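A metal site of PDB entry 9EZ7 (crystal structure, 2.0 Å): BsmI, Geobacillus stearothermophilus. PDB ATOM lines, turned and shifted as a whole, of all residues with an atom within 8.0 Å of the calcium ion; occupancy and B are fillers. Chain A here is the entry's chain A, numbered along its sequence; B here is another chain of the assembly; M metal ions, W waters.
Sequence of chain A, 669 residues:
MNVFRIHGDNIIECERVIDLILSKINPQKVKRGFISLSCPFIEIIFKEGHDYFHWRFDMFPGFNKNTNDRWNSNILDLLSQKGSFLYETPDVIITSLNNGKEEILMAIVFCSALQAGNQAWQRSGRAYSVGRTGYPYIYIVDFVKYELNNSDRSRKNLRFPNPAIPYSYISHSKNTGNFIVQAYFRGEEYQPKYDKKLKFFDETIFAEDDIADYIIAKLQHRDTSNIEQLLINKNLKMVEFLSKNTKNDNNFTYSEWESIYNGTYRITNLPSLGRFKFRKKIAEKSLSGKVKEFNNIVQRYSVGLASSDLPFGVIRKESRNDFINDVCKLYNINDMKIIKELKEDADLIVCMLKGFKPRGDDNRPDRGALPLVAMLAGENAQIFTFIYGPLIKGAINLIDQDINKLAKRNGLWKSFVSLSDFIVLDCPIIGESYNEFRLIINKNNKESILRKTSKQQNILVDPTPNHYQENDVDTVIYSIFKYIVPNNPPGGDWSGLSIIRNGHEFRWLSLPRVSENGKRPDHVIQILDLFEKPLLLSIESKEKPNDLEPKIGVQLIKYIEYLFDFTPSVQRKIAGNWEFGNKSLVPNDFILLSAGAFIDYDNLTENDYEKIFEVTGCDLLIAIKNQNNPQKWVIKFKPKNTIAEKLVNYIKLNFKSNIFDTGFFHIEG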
ATOM      1  N   GLU A 470     -11.454   5.320  12.533  1.00  0.00           N
ATOM      2  CA  GLU A 470     -12.907   5.142  12.494  1.00  0.00           C
ATOM      3  C   GLU A 470     -13.474   4.212  13.569  1.00  0.00           C
ATOM      4  O   GLU A 470     -14.490   4.568  14.157  1.00  0.00           O
ATOM      5  CB  GLU A 470     -13.403   4.704  11.109  1.00  0.00           C
ATOM      6  CG  GLU A 470     -14.842   5.096  10.856  1.00  0.00           C
ATOM      7  CD  GLU A 470     -15.349   4.795   9.456  1.00  0.00           C
ATOM      8  OE1 GLU A 470     -14.824   5.396   8.496  1.00  0.00           O
ATOM      9  OE2 GLU A 470     -16.302   3.994   9.324  1.00  0.00           O
ATOM     10  N   ASN A 471     -12.812   3.062  13.857  1.00  0.00           N
ATOM     11  CA  ASN A 471     -13.237   2.123  14.915  1.00  0.00           C
ATOM     12  C   ASN A 471     -13.355   2.864  16.267  1.00  0.00           C
ATOM     13  O   ASN A 471     -14.306   2.641  17.001  1.00  0.00           O
ATOM     14  CB  ASN A 471     -12.187   1.004  15.106  1.00  0.00           C
ATOM     15  CG  ASN A 471     -12.302  -0.143  14.151  1.00  0.00           C
ATOM     16  OD1 ASN A 471     -11.410  -0.349  13.306  1.00  0.00           O
ATOM     17  ND2 ASN A 471     -13.387  -0.919  14.306  1.00  0.00           N
ATOM     18  N   VAL A 473     -13.784   6.176  16.751  1.00  0.00           N
ATOM     19  CA  VAL A 473     -14.900   7.131  16.682  1.00  0.00           C
ATOM     20  C   VAL A 473     -16.193   6.397  17.043  1.00  0.00           C
ATOM     21  O   VAL A 473     -16.976   6.895  17.854  1.00  0.00           O
ATOM     22  CB  VAL A 473     -14.991   7.792  15.276  1.00  0.00           C
ATOM     23  CG1 VAL A 473     -16.239   8.674  15.170  1.00  0.00           C
ATOM     24  CG2 VAL A 473     -13.735   8.611  14.977  1.00  0.00           C
ATOM     25  N   ASP A 474     -16.414   5.191  16.463  1.00  0.00           N
ATOM     26  CA  ASP A 474     -17.610   4.410  16.745  1.00  0.00           C
ATOM     27  C   ASP A 474     -17.667   3.950  18.196  1.00  0.00           C
ATOM     28  O   ASP A 474     -18.739   3.955  18.796  1.00  0.00           O
ATOM     29  CB  ASP A 474     -17.731   3.193  15.797  1.00  0.00           C
ATOM     30  CG  ASP A 474     -18.169   3.596  14.411  1.00  0.00           C
ATOM     31  OD1 ASP A 474     -19.046   4.506  14.296  1.00  0.00           O
ATOM     32  OD2 ASP A 474     -17.657   3.013  13.418  1.00  0.00           O
ATOM     33  N   ARG A 520     -27.461   4.636   4.711  1.00  0.00           N
ATOM     34  CA  ARG A 520     -27.732   4.022   5.999  1.00  0.00           C
ATOM     35  C   ARG A 520     -26.841   4.606   7.091  1.00  0.00           C
ATOM     36  O   ARG A 520     -25.627   4.569   6.953  1.00  0.00           O
ATOM     37  CB  ARG A 520     -27.536   2.492   5.906  1.00  0.00           C
ATOM     38  CG  ARG A 520     -27.840   1.732   7.186  1.00  0.00           C
ATOM     39  CD  ARG A 520     -27.673   0.246   6.955  1.00  0.00           C
ATOM     40  NE  ARG A 520     -26.258  -0.119   6.819  1.00  0.00           N
ATOM     41  CZ  ARG A 520     -25.827  -1.186   6.153  1.00  0.00           C
ATOM     42  NH1 ARG A 520     -26.683  -1.986   5.533  1.00  0.00           N
ATOM     43  NH2 ARG A 520     -24.527  -1.453   6.088  1.00  0.00           N
ATOM     44  N   PRO A 521     -27.426   5.176   8.171  1.00  0.00           N
ATOM     45  CA  PRO A 521     -26.584   5.758   9.232  1.00  0.00           C
ATOM     46  C   PRO A 521     -25.783   4.717   9.990  1.00  0.00           C
ATOM     47  O   PRO A 521     -26.215   3.593  10.148  1.00  0.00           O
ATOM     48  CB  PRO A 521     -27.596   6.452  10.165  1.00  0.00           C
ATOM     49  CG  PRO A 521     -28.887   6.493   9.420  1.00  0.00           C
ATOM     50  CD  PRO A 521     -28.861   5.336   8.468  1.00  0.00           C
ATOM     51  N   ASP A 522     -24.608   5.109  10.481  1.00  0.00           N
ATOM     52  CA  ASP A 522     -23.767   4.233  11.277  1.00  0.00           C
ATOM     53  C   ASP A 522     -24.358   4.002  12.662  1.00  0.00           C
ATOM     54  O   ASP A 522     -24.209   2.907  13.218  1.00  0.00           O
ATOM     55  CB  ASP A 522     -22.353   4.837  11.393  1.00  0.00           C
ATOM     56  CG  ASP A 522     -21.632   4.849  10.082  1.00  0.00           C
ATOM     57  OD1 ASP A 522     -21.907   3.958   9.244  1.00  0.00           O
ATOM     58  OD2 ASP A 522     -20.785   5.724   9.875  1.00  0.00           O
ATOM     59  N   HIS A 523     -25.044   5.023  13.208  1.00  0.00           N
ATOM     60  CA  HIS A 523     -25.727   4.965  14.508  1.00  0.00           C
ATOM     61  C   HIS A 523     -26.995   5.776  14.418  1.00  0.00           C
ATOM     62  O   HIS A 523     -27.011   6.842  13.804  1.00  0.00           O
ATOM     63  CB  HIS A 523     -24.908   5.631  15.632  1.00  0.00           C
ATOM     64  CG  HIS A 523     -23.473   5.227  15.715  1.00  0.00           C
ATOM     65  ND1 HIS A 523     -23.040   4.237  16.595  1.00  0.00           N
ATOM     66  CD2 HIS A 523     -22.390   5.721  15.056  1.00  0.00           C
ATOM     67  CE1 HIS A 523     -21.736   4.159  16.428  1.00  0.00           C
ATOM     68  NE2 HIS A 523     -21.299   5.013  15.506  1.00  0.00           N
ATOM     69  N   ILE A 539     -26.116   9.392  12.910  1.00  0.00           N
ATOM     70  CA  ILE A 539     -24.714   9.739  12.925  1.00  0.00           C
ATOM     71  C   ILE A 539     -23.905   8.950  11.902  1.00  0.00           C
ATOM     72  O   ILE A 539     -24.019   7.735  11.815  1.00  0.00           O
ATOM     73  CB  ILE A 539     -24.110   9.556  14.346  1.00  0.00           C
ATOM     74  CG1 ILE A 539     -24.981  10.210  15.452  1.00  0.00           C
ATOM     75  CG2 ILE A 539     -22.642  10.035  14.439  1.00  0.00           C
ATOM     76  CD1 ILE A 539     -24.576   9.845  16.849  1.00  0.00           C
ATOM     77  N   GLU A 540     -23.045   9.650  11.166  1.00  0.00           N
ATOM     78  CA  GLU A 540     -22.113   9.031  10.263  1.00  0.00           C
ATOM     79  C   GLU A 540     -20.714   9.244  10.873  1.00  0.00           C
ATOM     80  O   GLU A 540     -20.359  10.371  11.233  1.00  0.00           O
ATOM     81  CB  GLU A 540     -22.231   9.630   8.875  1.00  0.00           C
ATOM     82  CG  GLU A 540     -21.172   9.161   7.902  1.00  0.00           C
ATOM     83  CD  GLU A 540     -21.541   7.911   7.126  1.00  0.00           C
ATOM     84  OE1 GLU A 540     -22.447   7.165   7.568  1.00  0.00           O
ATOM     85  OE2 GLU A 540     -20.935   7.688   6.052  1.00  0.00           O
ATOM     86  N   SER A 541     -19.944   8.162  11.037  1.00  0.00           N
ATOM     87  CA  SER A 541     -18.608   8.281  11.611  1.00  0.00           C
ATOM     88  C   SER A 541     -17.516   8.119  10.543  1.00  0.00           C
ATOM     89  O   SER A 541     -17.602   7.272   9.662  1.00  0.00           O
ATOM     90  CB  SER A 541     -18.418   7.237  12.702  1.00  0.00           C
ATOM     91  OG  SER A 541     -18.568   5.947  12.130  1.00  0.00           O
ATOM     92  N   LYS A 542     -16.487   8.960  10.619  1.00  0.00           N
ATOM     93  CA  LYS A 542     -15.360   8.931   9.699  1.00  0.00           C
ATOM     94  C   LYS A 542     -14.065   9.142  10.505  1.00  0.00           C
ATOM     95  O   LYS A 542     -14.087   9.668  11.609  1.00  0.00           O
ATOM     96  CB  LYS A 542     -15.488  10.054   8.643  1.00  0.00           C
ATOM     97  CG  LYS A 542     -16.600   9.845   7.631  1.00  0.00           C
ATOM     98  CD  LYS A 542     -16.323   8.651   6.745  1.00  0.00           C
ATOM     99  CE  LYS A 542     -17.441   8.463   5.764  1.00  0.00           C
ATOM    100  NZ  LYS A 542     -17.103   7.470   4.728  1.00  0.00           N
ATOM    101  N   GLU A 543     -12.919   8.740   9.939  1.00  0.00           N
ATOM    102  CA  GLU A 543     -11.627   8.952  10.586  1.00  0.00           C
ATOM    103  C   GLU A 543     -11.327  10.447  10.600  1.00  0.00           C
ATOM    104  O   GLU A 543     -10.985  10.983  11.655  1.00  0.00           O
ATOM    105  CB  GLU A 543     -10.521   8.176   9.872  1.00  0.00           C
ATOM    106  CG  GLU A 543      -9.137   8.442  10.413  1.00  0.00           C
ATOM    107  CD  GLU A 543      -8.019   7.648   9.769  1.00  0.00           C
ATOM    108  OE1 GLU A 543      -8.294   6.905   8.797  1.00  0.00           O
ATOM    109  OE2 GLU A 543      -6.858   7.765  10.227  1.00  0.00           O
ATOM    110  N   LEU A 548     -16.171  13.146   5.255  1.00  0.00           N
ATOM    111  CA  LEU A 548     -17.625  13.322   5.222  1.00  0.00           C
ATOM    112  C   LEU A 548     -18.016  13.779   3.819  1.00  0.00           C
ATOM    113  O   LEU A 548     -17.609  14.848   3.367  1.00  0.00           O
ATOM    114  CB  LEU A 548     -18.085  14.317   6.285  1.00  0.00           C
ATOM    115  CG  LEU A 548     -17.902  13.852   7.741  1.00  0.00           C
ATOM    116  CD1 LEU A 548     -18.047  15.025   8.710  1.00  0.00           C
ATOM    117  CD2 LEU A 548     -18.869  12.739   8.075  1.00  0.00           C
ATOM    118  N   ALA A 597     -19.321  12.547  12.811  1.00  0.00           N
ATOM    119  CA  ALA A 597     -18.345  12.387  13.883  1.00  0.00           C
ATOM    120  C   ALA A 597     -16.983  12.012  13.294  1.00  0.00           C
ATOM    121  O   ALA A 597     -16.924  11.279  12.322  1.00  0.00           O
ATOM    122  CB  ALA A 597     -18.814  11.320  14.864  1.00  0.00           C
ATOM    123  P    DG B  11     -18.752   2.889  -0.327  1.00  0.00           P
ATOM    124  OP1  DG B  11     -19.860   3.425   0.516  1.00  0.00           O
ATOM    125  OP2  DG B  11     -18.173   3.698  -1.427  1.00  0.00           O
ATOM    126  O5'  DG B  11     -17.553   2.462   0.619  1.00  0.00           O
ATOM    127  C5'  DG B  11     -17.704   1.341   1.477  1.00  0.00           C
ATOM    128  C4'  DG B  11     -16.341   0.854   1.924  1.00  0.00           C
ATOM    129  O4'  DG B  11     -15.774  -0.023   0.900  1.00  0.00           O
ATOM    130  C3'  DG B  11     -15.304   1.949   2.162  1.00  0.00           C
ATOM    131  O3'  DG B  11     -14.625   1.665   3.340  1.00  0.00           O
ATOM    132  C2'  DG B  11     -14.394   1.858   0.932  1.00  0.00           C
ATOM    133  C1'  DG B  11     -14.453   0.365   0.624  1.00  0.00           C
ATOM    134  N9   DG B  11     -14.152   0.044  -0.774  1.00  0.00           N
ATOM    135  C8   DG B  11     -14.563   0.703  -1.898  1.00  0.00           C
ATOM    136  N7   DG B  11     -14.182   0.129  -3.014  1.00  0.00           N
ATOM    137  C5   DG B  11     -13.493  -1.001  -2.594  1.00  0.00           C
ATOM    138  C6   DG B  11     -12.860  -2.037  -3.342  1.00  0.00           C
ATOM    139  O6   DG B  11     -12.745  -2.138  -4.575  1.00  0.00           O
ATOM    140  N1   DG B  11     -12.273  -2.986  -2.517  1.00  0.00           N
ATOM    141  C2   DG B  11     -12.327  -2.968  -1.145  1.00  0.00           C
ATOM    142  N2   DG B  11     -11.711  -3.967  -0.511  1.00  0.00           N
ATOM    143  N3   DG B  11     -12.939  -2.031  -0.430  1.00  0.00           N
ATOM    144  C4   DG B  11     -13.477  -1.080  -1.215  1.00  0.00           C
ATOM    145  P    DA B  12     -13.831   2.817   4.134  1.00  0.00           P
ATOM    146  OP1  DA B  12     -14.440   2.900   5.493  1.00  0.00           O
ATOM    147  OP2  DA B  12     -13.738   4.021   3.269  1.00  0.00           O
ATOM    148  O5'  DA B  12     -12.381   2.161   4.256  1.00  0.00           O
ATOM    149  C5'  DA B  12     -12.291   0.745   4.467  1.00  0.00           C
ATOM    150  C4'  DA B  12     -10.987   0.188   3.928  1.00  0.00           C
ATOM    151  O4'  DA B  12     -11.111  -0.128   2.519  1.00  0.00           O
ATOM    152  C3'  DA B  12      -9.782   1.126   4.064  1.00  0.00           C
ATOM    153  O3'  DA B  12      -8.767   0.453   4.804  1.00  0.00           O
ATOM    154  C2'  DA B  12      -9.369   1.417   2.616  1.00  0.00           C
ATOM    155  C1'  DA B  12      -9.926   0.217   1.857  1.00  0.00           C
ATOM    156  N9   DA B  12     -10.231   0.497   0.438  1.00  0.00           N
ATOM    157  C8   DA B  12     -10.916   1.567  -0.064  1.00  0.00           C
ATOM    158  N7   DA B  12     -11.026   1.551  -1.380  1.00  0.00           N
ATOM    159  C5   DA B  12     -10.361   0.403  -1.762  1.00  0.00           C
ATOM    160  C6   DA B  12     -10.098  -0.176  -3.022  1.00  0.00           C
ATOM    161  N6   DA B  12     -10.525   0.350  -4.173  1.00  0.00           N
ATOM    162  N1   DA B  12      -9.369  -1.303  -3.051  1.00  0.00           N
ATOM    163  C2   DA B  12      -8.949  -1.835  -1.901  1.00  0.00           C
ATOM    164  N3   DA B  12      -9.153  -1.402  -0.646  1.00  0.00           N
ATOM    165  C4   DA B  12      -9.851  -0.262  -0.656  1.00  0.00           C
HETATM  166 CA    CA M   1     -18.452   4.995   9.337  1.00  0.00          CA
HETATM  167  O   HOH W   1     -18.535   3.246  10.910  1.00  0.00           O
HETATM  168  O   HOH W   2     -18.865   5.788   7.318  1.00  0.00           O
HETATM  169  O   HOH W   3     -19.263   3.045   8.177  1.00  0.00           O
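The side-chain carboxylate of Asp 474 lies within hydrogen-bond range of the side-chain hydroxyl of Ser 541 (2.6 Å). N of Asp 522 lies within hydrogen-bond range of O of Ile 539 (3.0 Å).
Three residues have an atom within 4 Å of the calcium ion: Glu 470, Asp 522 and Ser 541.
Water W2 binds the calcium ion (2.2 Å). The calcium ion is bound by water W1. The side-chain carboxylate (OE2) of Glu 470 binds the calcium ion (2.4 Å). The calcium ion is bound by water W3 (2.4 Å). The calcium ion is bound by the backbone carbonyl oxygen (O) of Ser 541 (2.5 Å). The calcium ion is bound by OD2 of Asp 522, 2.5 Å away. The calcium ion has six donor atoms within binding distance. Slightly farther from the calcium ion lies the side-chain hydroxyl (OG) of Ser 541 (3.0 Å).
Water W1 lies within hydrogen-bond range of OD2 of Asp 474 (2.7 Å) and OG of Ser 541 (3.0 Å).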
